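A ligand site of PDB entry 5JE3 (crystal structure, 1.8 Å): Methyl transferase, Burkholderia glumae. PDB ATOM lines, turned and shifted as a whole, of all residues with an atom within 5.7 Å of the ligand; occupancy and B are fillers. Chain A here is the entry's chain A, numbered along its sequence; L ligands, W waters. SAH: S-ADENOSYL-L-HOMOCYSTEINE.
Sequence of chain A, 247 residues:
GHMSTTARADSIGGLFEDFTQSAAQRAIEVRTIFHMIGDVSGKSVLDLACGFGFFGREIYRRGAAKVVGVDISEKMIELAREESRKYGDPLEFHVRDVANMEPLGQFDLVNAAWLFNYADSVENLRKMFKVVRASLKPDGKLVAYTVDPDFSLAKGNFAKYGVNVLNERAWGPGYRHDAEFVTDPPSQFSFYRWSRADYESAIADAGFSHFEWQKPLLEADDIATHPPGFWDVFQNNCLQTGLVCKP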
ATOM      1  N   ARG A  26      34.758  -3.615  15.108  1.00  0.00           N
ATOM      2  CA  ARG A  26      34.935  -3.168  16.480  1.00  0.00           C
ATOM      3  C   ARG A  26      35.307  -4.295  17.434  1.00  0.00           C
ATOM      4  O   ARG A  26      35.251  -4.109  18.664  1.00  0.00           O
ATOM      5  CB  ARG A  26      33.654  -2.485  16.983  1.00  0.00           C
ATOM      6  CG  ARG A  26      33.145  -1.379  16.069  1.00  0.00           C
ATOM      7  CD  ARG A  26      32.045  -0.561  16.737  1.00  0.00           C
ATOM      8  NE  ARG A  26      32.519   0.208  17.884  1.00  0.00           N
ATOM      9  CZ  ARG A  26      31.756   1.032  18.620  1.00  0.00           C
ATOM     10  NH1 ARG A  26      30.470   1.192  18.325  1.00  0.00           N
ATOM     11  NH2 ARG A  26      32.279   1.690  19.637  1.00  0.00           N
ATOM     12  N   GLU A  29      37.928  -3.555  20.075  1.00  0.00           N
ATOM     13  CA  GLU A  29      37.454  -2.529  20.993  1.00  0.00           C
ATOM     14  C   GLU A  29      36.453  -3.090  21.985  1.00  0.00           C
ATOM     15  O   GLU A  29      36.560  -2.853  23.201  1.00  0.00           O
ATOM     16  CB  GLU A  29      36.844  -1.387  20.194  1.00  0.00           C
ATOM     17  CG  GLU A  29      35.985  -0.452  21.028  1.00  0.00           C
ATOM     18  CD  GLU A  29      35.380   0.661  20.196  1.00  0.00           C
ATOM     19  OE1 GLU A  29      35.427   0.584  18.941  1.00  0.00           O
ATOM     20  OE2 GLU A  29      34.840   1.617  20.789  1.00  0.00           O
ATOM     21  N   ASP A  47      26.317   4.999  30.994  1.00  0.00           N
ATOM     22  CA  ASP A  47      27.025   4.936  29.703  1.00  0.00           C
ATOM     23  C   ASP A  47      27.057   6.345  29.105  1.00  0.00           C
ATOM     24  O   ASP A  47      26.061   6.810  28.569  1.00  0.00           O
ATOM     25  CB  ASP A  47      26.308   3.939  28.779  1.00  0.00           C
ATOM     26  CG  ASP A  47      27.102   3.590  27.505  1.00  0.00           C
ATOM     27  OD1 ASP A  47      28.344   3.587  27.561  1.00  0.00           O
ATOM     28  OD2 ASP A  47      26.465   3.294  26.461  1.00  0.00           O
ATOM     29  N   LEU A  48      28.220   7.019  29.205  1.00  0.00           N
ATOM     30  CA  LEU A  48      28.377   8.394  28.737  1.00  0.00           C
ATOM     31  C   LEU A  48      28.803   8.431  27.271  1.00  0.00           C
ATOM     32  O   LEU A  48      29.539   7.550  26.807  1.00  0.00           O
ATOM     33  CB  LEU A  48      29.423   9.099  29.580  1.00  0.00           C
ATOM     34  CG  LEU A  48      29.070   9.207  31.068  1.00  0.00           C
ATOM     35  CD1 LEU A  48      30.183   9.968  31.770  1.00  0.00           C
ATOM     36  CD2 LEU A  48      27.703   9.914  31.252  1.00  0.00           C
ATOM     37  N   ALA A  49      28.347   9.466  26.558  1.00  0.00           N
ATOM     38  CA  ALA A  49      28.549   9.579  25.113  1.00  0.00           C
ATOM     39  C   ALA A  49      28.056   8.324  24.410  1.00  0.00           C
ATOM     40  O   ALA A  49      28.742   7.722  23.577  1.00  0.00           O
ATOM     41  CB  ALA A  49      30.015   9.879  24.759  1.00  0.00           C
ATOM     42  N   CYS A  50      26.824   7.923  24.753  1.00  0.00           N
ATOM     43  CA  CYS A  50      26.328   6.574  24.477  1.00  0.00           C
ATOM     44  C   CYS A  50      25.930   6.345  23.033  1.00  0.00           C
ATOM     45  O   CYS A  50      25.739   5.182  22.645  1.00  0.00           O
ATOM     46  CB  CYS A  50      25.122   6.268  25.372  1.00  0.00           C
ATOM     47  SG  CYS A  50      23.642   7.322  25.120  1.00  0.00           S
ATOM     48  N   GLY A  51      25.795   7.397  22.220  1.00  0.00           N
ATOM     49  CA  GLY A  51      25.348   7.191  20.852  1.00  0.00           C
ATOM     50  C   GLY A  51      23.954   6.582  20.846  1.00  0.00           C
ATOM     51  O   GLY A  51      23.074   6.976  21.622  1.00  0.00           O
ATOM     52  N   PHE A  52      23.737   5.602  19.961  1.00  0.00           N
ATOM     53  CA  PHE A  52      22.469   4.882  19.981  1.00  0.00           C
ATOM     54  C   PHE A  52      22.397   3.852  21.108  1.00  0.00           C
ATOM     55  O   PHE A  52      21.398   3.114  21.182  1.00  0.00           O
ATOM     56  CB  PHE A  52      22.180   4.232  18.621  1.00  0.00           C
ATOM     57  CG  PHE A  52      23.167   3.167  18.222  1.00  0.00           C
ATOM     58  CD1 PHE A  52      23.060   1.873  18.716  1.00  0.00           C
ATOM     59  CD2 PHE A  52      24.191   3.445  17.331  1.00  0.00           C
ATOM     60  CE1 PHE A  52      23.976   0.871  18.336  1.00  0.00           C
ATOM     61  CE2 PHE A  52      25.109   2.466  16.948  1.00  0.00           C
ATOM     62  CZ  PHE A  52      25.000   1.187  17.459  1.00  0.00           C
ATOM     63  N   PHE A  54      24.967   1.443  22.121  1.00  0.00           N
ATOM     64  CA  PHE A  54      25.576   0.137  21.866  1.00  0.00           C
ATOM     65  C   PHE A  54      26.122  -0.510  23.143  1.00  0.00           C
ATOM     66  O   PHE A  54      25.734  -1.627  23.491  1.00  0.00           O
ATOM     67  CB  PHE A  54      26.688   0.271  20.813  1.00  0.00           C
ATOM     68  CG  PHE A  54      27.422  -1.026  20.561  1.00  0.00           C
ATOM     69  CD1 PHE A  54      26.872  -1.995  19.757  1.00  0.00           C
ATOM     70  CD2 PHE A  54      28.636  -1.278  21.181  1.00  0.00           C
ATOM     71  CE1 PHE A  54      27.525  -3.194  19.539  1.00  0.00           C
ATOM     72  CE2 PHE A  54      29.298  -2.468  20.975  1.00  0.00           C
ATOM     73  CZ  PHE A  54      28.742  -3.427  20.143  1.00  0.00           C
ATOM     74  N   PHE A  55      27.015   0.186  23.859  1.00  0.00           N
ATOM     75  CA  PHE A  55      27.665  -0.438  25.018  1.00  0.00           C
ATOM     76  C   PHE A  55      26.699  -0.609  26.195  1.00  0.00           C
ATOM     77  O   PHE A  55      26.693  -1.660  26.838  1.00  0.00           O
ATOM     78  CB  PHE A  55      28.898   0.359  25.451  1.00  0.00           C
ATOM     79  CG  PHE A  55      30.074   0.060  24.587  1.00  0.00           C
ATOM     80  CD1 PHE A  55      30.688  -1.173  24.685  1.00  0.00           C
ATOM     81  CD2 PHE A  55      30.482   0.945  23.616  1.00  0.00           C
ATOM     82  CE1 PHE A  55      31.747  -1.497  23.832  1.00  0.00           C
ATOM     83  CE2 PHE A  55      31.526   0.641  22.785  1.00  0.00           C
ATOM     84  CZ  PHE A  55      32.168  -0.576  22.892  1.00  0.00           C
ATOM     85  N   VAL A  70      23.729   8.612  28.338  1.00  0.00           N
ATOM     86  CA  VAL A  70      23.750  10.069  28.143  1.00  0.00           C
ATOM     87  C   VAL A  70      24.491  10.392  26.861  1.00  0.00           C
ATOM     88  O   VAL A  70      25.604   9.884  26.628  1.00  0.00           O
ATOM     89  CB  VAL A  70      24.436  10.783  29.313  1.00  0.00           C
ATOM     90  CG1 VAL A  70      24.565  12.328  29.033  1.00  0.00           C
ATOM     91  CG2 VAL A  70      23.658  10.536  30.577  1.00  0.00           C
ATOM     92  N   ASP A  71      23.930  11.295  26.073  1.00  0.00           N
ATOM     93  CA  ASP A  71      24.591  11.797  24.876  1.00  0.00           C
ATOM     94  C   ASP A  71      24.167  13.253  24.688  1.00  0.00           C
ATOM     95  O   ASP A  71      23.069  13.654  25.076  1.00  0.00           O
ATOM     96  CB  ASP A  71      24.229  10.947  23.649  1.00  0.00           C
ATOM     97  CG  ASP A  71      25.242  11.062  22.528  1.00  0.00           C
ATOM     98  OD1 ASP A  71      26.072  10.149  22.356  1.00  0.00           O
ATOM     99  OD2 ASP A  71      25.203  12.087  21.811  1.00  0.00           O
ATOM    100  N   ILE A  72      25.066  14.045  24.113  1.00  0.00           N
ATOM    101  CA  ILE A  72      24.757  15.453  23.877  1.00  0.00           C
ATOM    102  C   ILE A  72      23.794  15.644  22.721  1.00  0.00           C
ATOM    103  O   ILE A  72      23.120  16.683  22.646  1.00  0.00           O
ATOM    104  CB  ILE A  72      26.076  16.225  23.665  1.00  0.00           C
ATOM    105  CG1 ILE A  72      25.876  17.725  23.806  1.00  0.00           C
ATOM    106  CG2 ILE A  72      26.715  15.859  22.306  1.00  0.00           C
ATOM    107  CD1 ILE A  72      27.184  18.471  23.829  1.00  0.00           C
ATOM    108  N   SER A  73      23.678  14.647  21.836  1.00  0.00           N
ATOM    109  CA  SER A  73      22.900  14.763  20.605  1.00  0.00           C
ATOM    110  C   SER A  73      21.468  14.304  20.827  1.00  0.00           C
ATOM    111  O   SER A  73      21.233  13.146  21.185  1.00  0.00           O
ATOM    112  CB  SER A  73      23.537  13.931  19.495  1.00  0.00           C
ATOM    113  OG  SER A  73      22.605  13.691  18.449  1.00  0.00           O
ATOM    114  N   MET A  76      20.772  11.392  18.370  1.00  0.00           N
ATOM    115  CA  MET A  76      21.323  10.110  18.805  1.00  0.00           C
ATOM    116  C   MET A  76      20.459   9.505  19.909  1.00  0.00           C
ATOM    117  O   MET A  76      20.224   8.287  19.907  1.00  0.00           O
ATOM    118  CB  MET A  76      22.754  10.273  19.298  1.00  0.00           C
ATOM    119  CG  MET A  76      23.797  10.511  18.224  1.00  0.00           C
ATOM    120  SD  MET A  76      23.838   9.227  16.955  1.00  0.00           S
ATOM    121  CE  MET A  76      23.012  10.043  15.604  1.00  0.00           C
ATOM    122  N   ARG A  96      22.326  15.204  27.477  1.00  0.00           N
ATOM    123  CA  ARG A  96      23.074  16.113  28.339  1.00  0.00           C
ATOM    124  C   ARG A  96      24.479  16.283  27.780  1.00  0.00           C
ATOM    125  O   ARG A  96      25.004  15.401  27.108  1.00  0.00           O
ATOM    126  CB  ARG A  96      23.101  15.599  29.789  1.00  0.00           C
ATOM    127  CG  ARG A  96      21.865  16.042  30.567  1.00  0.00           C
ATOM    128  CD  ARG A  96      21.653  15.285  31.861  1.00  0.00           C
ATOM    129  NE  ARG A  96      20.233  15.143  32.161  1.00  0.00           N
ATOM    130  CZ  ARG A  96      19.763  14.836  33.367  1.00  0.00           C
ATOM    131  NH1 ARG A  96      20.596  14.685  34.374  1.00  0.00           N
ATOM    132  NH2 ARG A  96      18.463  14.704  33.562  1.00  0.00           N
ATOM    133  N   ASP A  97      25.097  17.433  28.074  1.00  0.00           N
ATOM    134  CA  ASP A  97      26.499  17.659  27.776  1.00  0.00           C
ATOM    135  C   ASP A  97      27.301  17.209  28.991  1.00  0.00           C
ATOM    136  O   ASP A  97      27.194  17.807  30.065  1.00  0.00           O
ATOM    137  CB  ASP A  97      26.737  19.137  27.434  1.00  0.00           C
ATOM    138  CG  ASP A  97      28.210  19.507  27.366  1.00  0.00           C
ATOM    139  OD1 ASP A  97      29.097  18.626  27.365  1.00  0.00           O
ATOM    140  OD2 ASP A  97      28.475  20.729  27.296  1.00  0.00           O
ATOM    141  N   VAL A  98      28.081  16.138  28.841  1.00  0.00           N
ATOM    142  CA  VAL A  98      28.759  15.556  29.998  1.00  0.00           C
ATOM    143  C   VAL A  98      29.633  16.585  30.684  1.00  0.00           C
ATOM    144  O   VAL A  98      29.795  16.562  31.913  1.00  0.00           O
ATOM    145  CB  VAL A  98      29.572  14.304  29.588  1.00  0.00           C
ATOM    146  CG1 VAL A  98      30.520  13.887  30.711  1.00  0.00           C
ATOM    147  CG2 VAL A  98      28.631  13.188  29.271  1.00  0.00           C
ATOM    148  N   ALA A  99      30.241  17.496  29.910  1.00  0.00           N
ATOM    149  CA  ALA A  99      31.122  18.475  30.533  1.00  0.00           C
ATOM    150  C   ALA A  99      30.366  19.374  31.490  1.00  0.00           C
ATOM    151  O   ALA A  99      30.951  19.911  32.437  1.00  0.00           O
ATOM    152  CB  ALA A  99      31.829  19.308  29.453  1.00  0.00           C
ATOM    153  N   ALA A 113      32.918   5.170  26.196  1.00  0.00           N
ATOM    154  CA  ALA A 113      33.590   4.786  24.953  1.00  0.00           C
ATOM    155  C   ALA A 113      33.484   5.970  23.982  1.00  0.00           C
ATOM    156  O   ALA A 113      32.404   6.241  23.454  1.00  0.00           O
ATOM    157  CB  ALA A 113      32.951   3.536  24.356  1.00  0.00           C
ATOM    158  N   TRP A 114      34.608   6.650  23.756  1.00  0.00           N
ATOM    159  CA  TRP A 114      34.703   7.797  22.840  1.00  0.00           C
ATOM    160  C   TRP A 114      33.963   9.013  23.381  1.00  0.00           C
ATOM    161  O   TRP A 114      33.241   9.691  22.654  1.00  0.00           O
ATOM    162  CB  TRP A 114      34.210   7.458  21.437  1.00  0.00           C
ATOM    163  CG  TRP A 114      34.923   6.296  20.910  1.00  0.00           C
ATOM    164  CD1 TRP A 114      34.408   5.035  20.703  1.00  0.00           C
ATOM    165  CD2 TRP A 114      36.319   6.220  20.605  1.00  0.00           C
ATOM    166  NE1 TRP A 114      35.404   4.201  20.242  1.00  0.00           N
ATOM    167  CE2 TRP A 114      36.576   4.899  20.163  1.00  0.00           C
ATOM    168  CE3 TRP A 114      37.371   7.158  20.621  1.00  0.00           C
ATOM    169  CZ2 TRP A 114      37.846   4.478  19.745  1.00  0.00           C
ATOM    170  CZ3 TRP A 114      38.634   6.738  20.227  1.00  0.00           C
ATOM    171  CH2 TRP A 114      38.865   5.403  19.798  1.00  0.00           C
ATOM    172  N   LEU A 115      34.155   9.283  24.675  1.00  0.00           N
ATOM    173  CA  LEU A 115      33.722  10.533  25.280  1.00  0.00           C
ATOM    174  C   LEU A 115      34.832  11.580  25.287  1.00  0.00           C
ATOM    175  O   LEU A 115      34.664  12.693  24.756  1.00  0.00           O
ATOM    176  CB  LEU A 115      33.248  10.279  26.724  1.00  0.00           C
ATOM    177  CG  LEU A 115      33.060  11.556  27.548  1.00  0.00           C
ATOM    178  CD1 LEU A 115      31.896  12.350  26.978  1.00  0.00           C
ATOM    179  CD2 LEU A 115      32.831  11.252  29.031  1.00  0.00           C
ATOM    180  N   TYR A 118      36.150  14.060  22.711  1.00  0.00           N
ATOM    181  CA  TYR A 118      35.311  15.154  22.273  1.00  0.00           C
ATOM    182  C   TYR A 118      35.434  16.386  23.163  1.00  0.00           C
ATOM    183  O   TYR A 118      34.824  17.414  22.838  1.00  0.00           O
ATOM    184  CB  TYR A 118      33.845  14.700  22.199  1.00  0.00           C
ATOM    185  CG  TYR A 118      33.662  13.811  21.021  1.00  0.00           C
ATOM    186  CD1 TYR A 118      33.520  14.330  19.745  1.00  0.00           C
ATOM    187  CD2 TYR A 118      33.728  12.428  21.176  1.00  0.00           C
ATOM    188  CE1 TYR A 118      33.405  13.499  18.657  1.00  0.00           C
ATOM    189  CE2 TYR A 118      33.615  11.588  20.084  1.00  0.00           C
ATOM    190  CZ  TYR A 118      33.449  12.125  18.832  1.00  0.00           C
ATOM    191  OH  TYR A 118      33.321  11.275  17.752  1.00  0.00           O
ATOM    192  N   MET A 128      35.012  17.020  32.504  1.00  0.00           N
ATOM    193  CA  MET A 128      34.398  15.718  32.254  1.00  0.00           C
ATOM    194  C   MET A 128      34.852  14.701  33.291  1.00  0.00           C
ATOM    195  O   MET A 128      34.042  13.929  33.796  1.00  0.00           O
ATOM    196  CB  MET A 128      34.721  15.194  30.855  1.00  0.00           C
ATOM    197  CG  MET A 128      33.984  15.905  29.727  1.00  0.00           C
ATOM    198  SD  MET A 128      34.504  15.161  28.154  1.00  0.00           S
ATOM    199  CE  MET A 128      33.436  16.039  27.030  1.00  0.00           C
HETATM  200  N   SAH L   1      29.659   5.224  22.869  1.00  0.00           N
HETATM  201  CA  SAH L   1      29.044   5.047  21.511  1.00  0.00           C
HETATM  202  CB  SAH L   1      29.160   6.301  20.618  1.00  0.00           C
HETATM  203  CG  SAH L   1      30.568   6.872  20.486  1.00  0.00           C
HETATM  204  SD  SAH L   1      30.541   8.137  19.217  1.00  0.00           S
HETATM  205  C   SAH L   1      29.718   3.885  20.853  1.00  0.00           C
HETATM  206  O   SAH L   1      29.100   3.209  20.029  1.00  0.00           O
HETATM  207  OXT SAH L   1      30.875   3.567  21.147  1.00  0.00           O
HETATM  208  C5' SAH L   1      30.800   9.579  20.201  1.00  0.00           C
HETATM  209  C4' SAH L   1      29.501  10.102  20.805  1.00  0.00           C
HETATM  210  O4' SAH L   1      29.822  11.095  21.777  1.00  0.00           O
HETATM  211  C3' SAH L   1      28.557  10.789  19.811  1.00  0.00           C
HETATM  212  O3' SAH L   1      27.303  10.087  19.823  1.00  0.00           O
HETATM  213  C2' SAH L   1      28.396  12.206  20.328  1.00  0.00           C
HETATM  214  O2' SAH L   1      27.067  12.772  20.157  1.00  0.00           O
HETATM  215  C1' SAH L   1      28.774  12.050  21.792  1.00  0.00           C
HETATM  216  N9  SAH L   1      29.294  13.268  22.442  1.00  0.00           N
HETATM  217  C8  SAH L   1      30.192  14.132  21.958  1.00  0.00           C
HETATM  218  N7  SAH L   1      30.449  15.121  22.846  1.00  0.00           N
HETATM  219  C5  SAH L   1      29.708  14.879  23.938  1.00  0.00           C
HETATM  220  C6  SAH L   1      29.495  15.514  25.250  1.00  0.00           C
HETATM  221  N6  SAH L   1      30.141  16.658  25.578  1.00  0.00           N
HETATM  222  N1  SAH L   1      28.616  14.944  26.107  1.00  0.00           N
HETATM  223  C2  SAH L   1      27.955  13.815  25.789  1.00  0.00           C
HETATM  224  N3  SAH L   1      28.113  13.184  24.614  1.00  0.00           N
HETATM  225  C4  SAH L   1      28.949  13.649  23.664  1.00  0.00           C
HETATM  226  O   HOH W   1      28.546   4.275  17.219  1.00  0.00           O
HETATM  227  O   HOH W   2      31.035  17.519  21.647  1.00  0.00           O
HETATM  228  O   HOH W   3      32.071  18.435  24.165  1.00  0.00           O
HETATM  229  O   HOH W   4      26.148   3.406  20.064  1.00  0.00           O
HETATM  230  O   HOH W   5      27.271  15.182  18.690  1.00  0.00           O
HETATM  231  O   HOH W   6      27.248   8.453  17.743  1.00  0.00           O
HETATM  232  O   HOH W   7      27.465   3.203  23.956  1.00  0.00           O
HETATM  233  O   HOH W   8      30.059   5.028  25.801  1.00  0.00           O
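Residues that only touch the ligand: Phe 55 (3.4 Å), Tyr 118 (3.5 Å), Trp 114 (3.5 Å), Cys 50 (3.5 Å), Arg 96 (3.6 Å), Gly 51 (3.6 Å), Met 128 (3.7 Å), Ser 73 (3.8 Å), Met 76 (3.9 Å) and Phe 54 (3.9 Å). Hydrophobic or aromatic side chains that line the ligand: Ala 49, Phe 54, Phe 55, Ile 72, Met 76, Val 98, Ala 113, Trp 114, Tyr 118 and Met 128. Of the 24 residues printed, 17 come within 4 Å of the ligand. The nearest printed residue that does not touch the ligand is Leu 115 (4.3 Å).
A nitrogen (N) of the ligand lies within hydrogen-bond range of the backbone carbonyl oxygen of Ala 49. The backbone NH (N) of Ile 72 sits at hydrogen-bond distance from a nitrogen (N3) of the ligand. OD2 of Asp 71 sits at hydrogen-bond distance from O2' of the ligand. The guanidinium group (NH2) of Arg 26 lies within salt-bridge range of an oxygen (OXT) of the ligand. The backbone NH (N) of Val 98 is in hydrogen-bond range of a nitrogen (N1) of the ligand, 3.0 Å away. The side-chain carboxylate of Asp 97 is in hydrogen-bond range of a nitrogen (N6) of the ligand. O of Ala 113 lies within hydrogen-bond range of N of the ligand (3.0 Å).
OD1 of Asp 71 sits at hydrogen-bond distance from N of Cys 50 (3.4 Å). The side-chain carboxylate (OD1) of Asp 71 is in hydrogen-bond range of the backbone NH (N) of Gly 51, at 2.8 Å. OD2 of Asp 71 lies within hydrogen-bond range of N of Ser 73 (3.0 Å). The backbone carbonyl oxygen (O) of Asp 71 sits at hydrogen-bond distance from the backbone NH (N) of Arg 96. OE2 of Glu 29 sits at hydrogen-bond distance from NE1 of Trp 114 (2.7 Å). The backbone NH (N) of Ala 99 sits at hydrogen-bond distance from the side-chain carboxylate (OD1) of Asp 97. N of Ala 49 is in hydrogen-bond range of O of Val 70 (2.8 Å). The side-chain hydroxyl (OG) of Ser 73 is in hydrogen-bond range of the backbone NH (N) of Met 76, 2.9 Å away.
Water W6 lies within hydrogen-bond range of O3' of the ligand (2.6 Å) and SD of Met 76 (3.6 Å). Water W4 lies within hydrogen-bond range of O of the ligand (3.0 Å), N of Phe 54 (3.1 Å), O of Cys 50 (3.2 Å) and N of Phe 52 (3.3 Å). Water W8 lies within hydrogen-bond range of O of Leu 48 (2.8 Å), OD1 of Asp 47 (2.8 Å), N of Ala 113 (2.9 Å) and N of the ligand (3.0 Å). Water W3 bridges N6 of the ligand (3.0 Å) and O of Tyr 118 (3.2 Å). Water W7 lies within hydrogen-bond range of OD2 of Asp 47 (2.7 Å), O of Cys 50 (2.9 Å), N of Phe 55 (3.1 Å) and N of the ligand (3.2 Å).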
